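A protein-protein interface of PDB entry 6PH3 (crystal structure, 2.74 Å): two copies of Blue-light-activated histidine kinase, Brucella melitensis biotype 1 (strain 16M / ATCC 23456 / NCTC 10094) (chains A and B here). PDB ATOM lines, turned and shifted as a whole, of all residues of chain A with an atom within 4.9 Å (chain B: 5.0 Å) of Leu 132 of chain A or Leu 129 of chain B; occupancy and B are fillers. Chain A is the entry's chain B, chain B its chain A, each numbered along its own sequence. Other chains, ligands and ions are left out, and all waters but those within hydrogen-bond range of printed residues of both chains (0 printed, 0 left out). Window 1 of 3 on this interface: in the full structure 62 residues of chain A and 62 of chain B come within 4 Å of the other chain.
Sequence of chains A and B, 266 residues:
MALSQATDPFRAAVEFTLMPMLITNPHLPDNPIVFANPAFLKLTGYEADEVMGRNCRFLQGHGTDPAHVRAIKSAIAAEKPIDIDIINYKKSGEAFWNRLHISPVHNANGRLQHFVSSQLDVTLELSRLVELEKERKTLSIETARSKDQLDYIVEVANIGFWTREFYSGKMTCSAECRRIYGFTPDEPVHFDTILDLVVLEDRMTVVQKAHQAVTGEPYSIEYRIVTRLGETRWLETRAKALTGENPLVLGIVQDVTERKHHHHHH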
ATOM      1  N   LEU A 124      -7.663 -19.660 -21.786  1.00  0.00           N
ATOM      2  CA  LEU A 124      -7.012 -20.605 -20.891  1.00  0.00           C
ATOM      3  C   LEU A 124      -7.609 -22.000 -21.037  1.00  0.00           C
ATOM      4  O   LEU A 124      -6.860 -22.949 -21.218  1.00  0.00           O
ATOM      5  CB  LEU A 124      -7.060 -20.162 -19.411  1.00  0.00           C
ATOM      6  CG  LEU A 124      -6.107 -19.057 -18.933  1.00  0.00           C
ATOM      7  CD1 LEU A 124      -6.290 -18.813 -17.473  1.00  0.00           C
ATOM      8  CD2 LEU A 124      -4.639 -19.448 -19.078  1.00  0.00           C
ATOM      9  N   ARG A 128      -4.682 -22.748 -23.773  1.00  0.00           N
ATOM     10  CA  ARG A 128      -3.578 -23.057 -22.846  1.00  0.00           C
ATOM     11  C   ARG A 128      -3.714 -24.433 -22.160  1.00  0.00           C
ATOM     12  O   ARG A 128      -2.740 -25.176 -22.136  1.00  0.00           O
ATOM     13  CB  ARG A 128      -3.356 -21.934 -21.808  1.00  0.00           C
ATOM     14  CG  ARG A 128      -2.152 -22.127 -20.872  1.00  0.00           C
ATOM     15  CD  ARG A 128      -0.807 -21.829 -21.520  1.00  0.00           C
ATOM     16  NE  ARG A 128       0.282 -21.841 -20.537  1.00  0.00           N
ATOM     17  CZ  ARG A 128       1.186 -22.812 -20.410  1.00  0.00           C
ATOM     18  NH1 ARG A 128       1.159 -23.865 -21.221  1.00  0.00           N
ATOM     19  NH2 ARG A 128       2.129 -22.732 -19.480  1.00  0.00           N
ATOM     20  N   LEU A 129      -4.899 -24.772 -21.613  1.00  0.00           N
ATOM     21  CA  LEU A 129      -5.177 -26.047 -20.957  1.00  0.00           C
ATOM     22  C   LEU A 129      -5.007 -27.190 -21.936  1.00  0.00           C
ATOM     23  O   LEU A 129      -4.393 -28.197 -21.562  1.00  0.00           O
ATOM     24  CB  LEU A 129      -6.584 -26.065 -20.318  1.00  0.00           C
ATOM     25  CG  LEU A 129      -7.225 -27.437 -19.996  1.00  0.00           C
ATOM     26  CD1 LEU A 129      -6.775 -27.964 -18.637  1.00  0.00           C
ATOM     27  CD2 LEU A 129      -8.743 -27.364 -20.060  1.00  0.00           C
ATOM     28  N   VAL A 130      -5.503 -27.038 -23.194  1.00  0.00           N
ATOM     29  CA  VAL A 130      -5.400 -28.113 -24.189  1.00  0.00           C
ATOM     30  C   VAL A 130      -3.922 -28.378 -24.548  1.00  0.00           C
ATOM     31  O   VAL A 130      -3.499 -29.526 -24.479  1.00  0.00           O
ATOM     32  CB  VAL A 130      -6.337 -27.967 -25.432  1.00  0.00           C
ATOM     33  CG1 VAL A 130      -7.725 -27.487 -25.038  1.00  0.00           C
ATOM     34  CG2 VAL A 130      -5.753 -27.087 -26.520  1.00  0.00           C
ATOM     35  N   GLU A 131      -3.132 -27.314 -24.834  1.00  0.00           N
ATOM     36  CA  GLU A 131      -1.719 -27.411 -25.213  1.00  0.00           C
ATOM     37  C   GLU A 131      -0.848 -27.927 -24.083  1.00  0.00           C
ATOM     38  O   GLU A 131       0.130 -28.608 -24.349  1.00  0.00           O
ATOM     39  CB  GLU A 131      -1.185 -26.084 -25.801  1.00  0.00           C
ATOM     40  CG  GLU A 131      -0.878 -24.987 -24.789  1.00  0.00           C
ATOM     41  CD  GLU A 131      -0.445 -23.620 -25.305  1.00  0.00           C
ATOM     42  OE1 GLU A 131      -0.971 -23.165 -26.351  1.00  0.00           O
ATOM     43  OE2 GLU A 131       0.373 -22.972 -24.609  1.00  0.00           O
ATOM     44  N   LEU A 132      -1.210 -27.608 -22.828  1.00  0.00           N
ATOM     45  CA  LEU A 132      -0.503 -28.020 -21.613  1.00  0.00           C
ATOM     46  C   LEU A 132      -0.781 -29.484 -21.290  1.00  0.00           C
ATOM     47  O   LEU A 132       0.087 -30.142 -20.724  1.00  0.00           O
ATOM     48  CB  LEU A 132      -0.883 -27.094 -20.444  1.00  0.00           C
ATOM     49  CG  LEU A 132      -0.033 -27.089 -19.165  1.00  0.00           C
ATOM     50  CD1 LEU A 132       1.465 -26.899 -19.456  1.00  0.00           C
ATOM     51  CD2 LEU A 132      -0.516 -26.021 -18.226  1.00  0.00           C
ATOM     52  N   GLU A 133      -1.956 -30.009 -21.674  1.00  0.00           N
ATOM     53  CA  GLU A 133      -2.230 -31.430 -21.493  1.00  0.00           C
ATOM     54  C   GLU A 133      -1.480 -32.233 -22.577  1.00  0.00           C
ATOM     55  O   GLU A 133      -0.740 -33.150 -22.216  1.00  0.00           O
ATOM     56  CB  GLU A 133      -3.735 -31.752 -21.434  1.00  0.00           C
ATOM     57  CG  GLU A 133      -4.065 -33.179 -20.989  1.00  0.00           C
ATOM     58  CD  GLU A 133      -3.122 -33.894 -20.026  1.00  0.00           C
ATOM     59  OE1 GLU A 133      -2.991 -33.444 -18.863  1.00  0.00           O
ATOM     60  OE2 GLU A 133      -2.538 -34.927 -20.432  1.00  0.00           O
ATOM     61  N   LYS A 134      -1.582 -31.832 -23.873  1.00  0.00           N
ATOM     62  CA  LYS A 134      -0.853 -32.461 -24.994  1.00  0.00           C
ATOM     63  C   LYS A 134       0.663 -32.536 -24.704  1.00  0.00           C
ATOM     64  O   LYS A 134       1.324 -33.458 -25.171  1.00  0.00           O
ATOM     65  CB  LYS A 134      -1.146 -31.740 -26.342  1.00  0.00           C
ATOM     66  CG  LYS A 134      -0.042 -30.800 -26.847  1.00  0.00           C
ATOM     67  CD  LYS A 134      -0.494 -29.766 -27.895  1.00  0.00           C
ATOM     68  CE  LYS A 134       0.548 -28.670 -28.122  1.00  0.00           C
ATOM     69  NZ  LYS A 134       0.086 -27.625 -29.085  1.00  0.00           N
ATOM     70  N   GLU A 135       1.187 -31.571 -23.915  1.00  0.00           N
ATOM     71  CA  GLU A 135       2.584 -31.436 -23.509  1.00  0.00           C
ATOM     72  C   GLU A 135       2.929 -32.417 -22.363  1.00  0.00           C
ATOM     73  O   GLU A 135       4.031 -32.972 -22.333  1.00  0.00           O
ATOM     74  CB  GLU A 135       2.835 -29.987 -23.098  1.00  0.00           C
ATOM     75  CG  GLU A 135       4.240 -29.649 -22.643  1.00  0.00           C
ATOM     76  CD  GLU A 135       4.441 -28.159 -22.439  1.00  0.00           C
ATOM     77  OE1 GLU A 135       4.389 -27.421 -23.452  1.00  0.00           O
ATOM     78  OE2 GLU A 135       4.665 -27.726 -21.283  1.00  0.00           O
ATOM     79  N   ARG A 136       1.983 -32.629 -21.436  1.00  0.00           N
ATOM     80  CA  ARG A 136       2.112 -33.540 -20.288  1.00  0.00           C
ATOM     81  C   ARG A 136       2.132 -34.998 -20.791  1.00  0.00           C
ATOM     82  O   ARG A 136       2.982 -35.778 -20.352  1.00  0.00           O
ATOM     83  CB  ARG A 136       0.949 -33.282 -19.295  1.00  0.00           C
ATOM     84  CG  ARG A 136       1.150 -33.796 -17.875  1.00  0.00           C
ATOM     85  CD  ARG A 136       0.016 -34.719 -17.488  1.00  0.00           C
ATOM     86  NE  ARG A 136       0.136 -36.030 -18.130  1.00  0.00           N
ATOM     87  CZ  ARG A 136      -0.776 -36.994 -18.053  1.00  0.00           C
ATOM     88  NH1 ARG A 136      -1.889 -36.811 -17.350  1.00  0.00           N
ATOM     89  NH2 ARG A 136      -0.585 -38.150 -18.678  1.00  0.00           N
ATOM     90  N   LEU B 124     -10.005 -23.212 -12.713  1.00  0.00           N
ATOM     91  CA  LEU B 124      -9.071 -23.673 -13.741  1.00  0.00           C
ATOM     92  C   LEU B 124      -7.742 -22.931 -13.638  1.00  0.00           C
ATOM     93  O   LEU B 124      -6.708 -23.575 -13.606  1.00  0.00           O
ATOM     94  CB  LEU B 124      -9.616 -23.532 -15.170  1.00  0.00           C
ATOM     95  CG  LEU B 124     -10.617 -24.536 -15.692  1.00  0.00           C
ATOM     96  CD1 LEU B 124     -11.103 -24.113 -17.082  1.00  0.00           C
ATOM     97  CD2 LEU B 124     -10.044 -25.958 -15.741  1.00  0.00           C
ATOM     98  N   GLU B 125      -7.774 -21.592 -13.520  1.00  0.00           N
ATOM     99  CA  GLU B 125      -6.569 -20.770 -13.440  1.00  0.00           C
ATOM    100  C   GLU B 125      -5.767 -20.985 -12.160  1.00  0.00           C
ATOM    101  O   GLU B 125      -4.570 -21.256 -12.252  1.00  0.00           O
ATOM    102  CB  GLU B 125      -6.941 -19.289 -13.577  1.00  0.00           C
ATOM    103  CG  GLU B 125      -5.764 -18.333 -13.678  1.00  0.00           C
ATOM    104  CD  GLU B 125      -6.141 -16.882 -13.450  1.00  0.00           C
ATOM    105  OE1 GLU B 125      -7.153 -16.417 -14.033  1.00  0.00           O
ATOM    106  OE2 GLU B 125      -5.394 -16.197 -12.715  1.00  0.00           O
ATOM    107  N   SER B 127      -6.158 -23.317  -9.658  1.00  0.00           N
ATOM    108  CA  SER B 127      -6.001 -24.680  -9.159  1.00  0.00           C
ATOM    109  C   SER B 127      -5.577 -25.691 -10.235  1.00  0.00           C
ATOM    110  O   SER B 127      -4.486 -26.245 -10.106  1.00  0.00           O
ATOM    111  CB  SER B 127      -7.255 -25.146  -8.421  1.00  0.00           C
ATOM    112  OG  SER B 127      -7.144 -24.926  -7.023  1.00  0.00           O
ATOM    113  N   ARG B 128      -6.388 -25.915 -11.303  1.00  0.00           N
ATOM    114  CA  ARG B 128      -6.041 -26.917 -12.308  1.00  0.00           C
ATOM    115  C   ARG B 128      -4.777 -26.562 -13.098  1.00  0.00           C
ATOM    116  O   ARG B 128      -3.875 -27.383 -13.182  1.00  0.00           O
ATOM    117  CB  ARG B 128      -7.222 -27.253 -13.226  1.00  0.00           C
ATOM    118  CG  ARG B 128      -6.988 -28.505 -14.065  1.00  0.00           C
ATOM    119  CD  ARG B 128      -8.281 -29.047 -14.633  1.00  0.00           C
ATOM    120  NE  ARG B 128      -8.098 -29.728 -15.919  1.00  0.00           N
ATOM    121  CZ  ARG B 128      -9.071 -29.948 -16.802  1.00  0.00           C
ATOM    122  NH1 ARG B 128     -10.306 -29.520 -16.562  1.00  0.00           N
ATOM    123  NH2 ARG B 128      -8.812 -30.575 -17.942  1.00  0.00           N
ATOM    124  N   LEU B 129      -4.684 -25.359 -13.630  1.00  0.00           N
ATOM    125  CA  LEU B 129      -3.528 -24.905 -14.384  1.00  0.00           C
ATOM    126  C   LEU B 129      -2.275 -24.998 -13.529  1.00  0.00           C
ATOM    127  O   LEU B 129      -1.262 -25.476 -14.037  1.00  0.00           O
ATOM    128  CB  LEU B 129      -3.751 -23.467 -14.911  1.00  0.00           C
ATOM    129  CG  LEU B 129      -2.512 -22.642 -15.339  1.00  0.00           C
ATOM    130  CD1 LEU B 129      -2.150 -22.891 -16.792  1.00  0.00           C
ATOM    131  CD2 LEU B 129      -2.719 -21.134 -15.065  1.00  0.00           C
ATOM    132  N   VAL B 130      -2.349 -24.599 -12.224  1.00  0.00           N
ATOM    133  CA  VAL B 130      -1.189 -24.640 -11.346  1.00  0.00           C
ATOM    134  C   VAL B 130      -0.750 -26.095 -11.105  1.00  0.00           C
ATOM    135  O   VAL B 130       0.429 -26.383 -11.269  1.00  0.00           O
ATOM    136  CB  VAL B 130      -1.296 -23.797 -10.040  1.00  0.00           C
ATOM    137  CG1 VAL B 130      -1.969 -22.456 -10.284  1.00  0.00           C
ATOM    138  CG2 VAL B 130      -1.957 -24.556  -8.893  1.00  0.00           C
ATOM    139  N   GLU B 131      -1.698 -27.012 -10.809  1.00  0.00           N
ATOM    140  CA  GLU B 131      -1.386 -28.421 -10.530  1.00  0.00           C
ATOM    141  C   GLU B 131      -0.863 -29.162 -11.762  1.00  0.00           C
ATOM    142  O   GLU B 131      -0.019 -30.038 -11.621  1.00  0.00           O
ATOM    143  CB  GLU B 131      -2.567 -29.163  -9.860  1.00  0.00           C
ATOM    144  CG  GLU B 131      -3.679 -29.593 -10.800  1.00  0.00           C
ATOM    145  CD  GLU B 131      -4.266 -30.968 -10.559  1.00  0.00           C
ATOM    146  OE1 GLU B 131      -5.422 -31.191 -10.991  1.00  0.00           O
ATOM    147  OE2 GLU B 131      -3.578 -31.826  -9.957  1.00  0.00           O
ATOM    148  N   LEU B 132      -1.340 -28.781 -12.958  1.00  0.00           N
ATOM    149  CA  LEU B 132      -0.897 -29.361 -14.221  1.00  0.00           C
ATOM    150  C   LEU B 132       0.524 -28.852 -14.546  1.00  0.00           C
ATOM    151  O   LEU B 132       1.304 -29.572 -15.160  1.00  0.00           O
ATOM    152  CB  LEU B 132      -1.914 -29.019 -15.327  1.00  0.00           C
ATOM    153  CG  LEU B 132      -1.762 -29.633 -16.730  1.00  0.00           C
ATOM    154  CD1 LEU B 132      -1.647 -31.121 -16.693  1.00  0.00           C
ATOM    155  CD2 LEU B 132      -2.958 -29.274 -17.588  1.00  0.00           C
ATOM    156  N   GLU B 133       0.856 -27.622 -14.100  1.00  0.00           N
ATOM    157  CA  GLU B 133       2.160 -26.984 -14.288  1.00  0.00           C
ATOM    158  C   GLU B 133       3.216 -27.633 -13.409  1.00  0.00           C
ATOM    159  O   GLU B 133       4.363 -27.746 -13.835  1.00  0.00           O
ATOM    160  CB  GLU B 133       2.084 -25.467 -14.022  1.00  0.00           C
ATOM    161  CG  GLU B 133       1.646 -24.664 -15.241  1.00  0.00           C
ATOM    162  CD  GLU B 133       1.358 -23.181 -15.062  1.00  0.00           C
ATOM    163  OE1 GLU B 133       0.947 -22.764 -13.953  1.00  0.00           O
ATOM    164  OE2 GLU B 133       1.489 -22.440 -16.065  1.00  0.00           O
ATOM    165  N   ARG B 136       3.914 -31.351 -14.689  1.00  0.00           N
ATOM    166  CA  ARG B 136       4.865 -31.421 -15.805  1.00  0.00           C
ATOM    167  C   ARG B 136       6.291 -31.117 -15.360  1.00  0.00           C
ATOM    168  O   ARG B 136       7.192 -31.680 -15.964  1.00  0.00           O
ATOM    169  CB  ARG B 136       4.459 -30.597 -17.046  1.00  0.00           C
ATOM    170  CG  ARG B 136       4.391 -29.089 -16.846  1.00  0.00           C
ATOM    171  CD  ARG B 136       4.776 -28.331 -18.100  1.00  0.00           C
ATOM    172  NE  ARG B 136       6.191 -28.501 -18.436  1.00  0.00           N
ATOM    173  CZ  ARG B 136       7.195 -27.872 -17.829  1.00  0.00           C
ATOM    174  NH1 ARG B 136       6.954 -27.016 -16.841  1.00  0.00           N
ATOM    175  NH2 ARG B 136       8.448 -28.098 -18.202  1.00  0.00           N
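Of the 10 printed residues of chain B, 6 touch a printed residue of chain A.
Hydrophobic or aromatic side chains of chain B that line the printed part of chain A: Leu 129 and Leu 132.
Hydrophobic or aromatic side chains of chain A that line the printed part of chain B: Leu 124, Leu 129 and Leu 132.
Among the printed residues, 9 pairs touch across the chains.
Among the printed residues, Asp or Glu carboxylates within 4 Å of a Lys or Arg side-chain nitrogen of the other chain: Arg 128 of chain A with Glu 133 of chain B (3.5 Å) and Glu 135 of chain A with Arg 136 of chain B (3.3 Å).
NH1 of Arg 128 of chain A is in salt-bridge range of OE2 of Glu 131 of chain A (3.6 Å).
The guanidinium group (NH1) of Arg 136 of chain A lies within salt-bridge range of the side-chain carboxylate (OE2) of Glu 133 of chain A (3.7 Å).
The backbone NH (N) of Leu 129 of chain B is in hydrogen-bond range of the backbone carbonyl oxygen (O) of Leu 124 of chain B (2.7 Å).
The backbone carbonyl oxygen (O) of Leu 124 of chain A sits at hydrogen-bond distance from the backbone NH (N) of Leu 129 of chain A (2.7 Å).
Leu 132 of chain A touches just these residues of chain B: Leu 129 (3.8 Å), Leu 132 (3.9 Å), Glu 133 (3.9 Å) and Arg 136 (3.9 Å).
Printed residues of chain A within 4 Å of Glu 125 of chain B: Leu 124.
Printed residues of chain B within 4 Å of Glu 133 of chain A: Leu 132.
Printed residues of chain B within 4 Å of Glu 135 of chain A: Arg 136.
The nearest printed residue of chain B that does not touch Leu 132 of chain A is Arg 128 of chain B (6.2 Å).
The nearest residue of chain A that does not touch Leu 129 of chain B is Arg 128 of chain A (4.2 Å).
The side-chain carboxylate (OE2) of Glu 135 of chain A is in salt-bridge range of the guanidinium group (NE) of Arg 136 of chain B, at 3.3 Å.
NH2 of Arg 128 of chain A lies within salt-bridge range of OE2 of Glu 133 of chain B, at 3.5 Å.
Arg 128 of chain A touches Glu 133 of chain B, but with the chains exchanged Glu 133 of chain A does not touch Arg 128 of chain B (6.2 Å).
Leu 132 of chain A touches Leu 129 of chain B, but with the chains exchanged Leu 129 of chain A does not touch Leu 132 of chain B (4.2 Å).
Leu 132 of chain A touches Glu 133 of chain B, and with the chains exchanged Glu 133 of chain A touches Leu 132 of chain B.
Leu 132 of chain A touches Arg 136 of chain B, but with the chains exchanged Arg 136 of chain A does not touch Leu 132 of chain B (4.04 Å).
Positions printed for both chains: 124, 128, 129, 130, 131, 132, 133 and 136.
Of the 9 pairs that touch across the chains among the printed residues, 3 have their exchanged pair printed and touching as well.
Among the printed residues, pairs that only touch across the chains: Leu 124 of chain A with Glu 125 of chain B, Leu 129 of chain A with Arg 128 of chain B, Leu 132 of chain A with Leu 129 of chain B, Leu 132 of chain A with Leu 132 of chain B, Leu 132 of chain A with Glu 133 of chain B, Leu 132 of chain A with Arg 136 of chain B and Glu 133 of chain A with Leu 132 of chain B.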
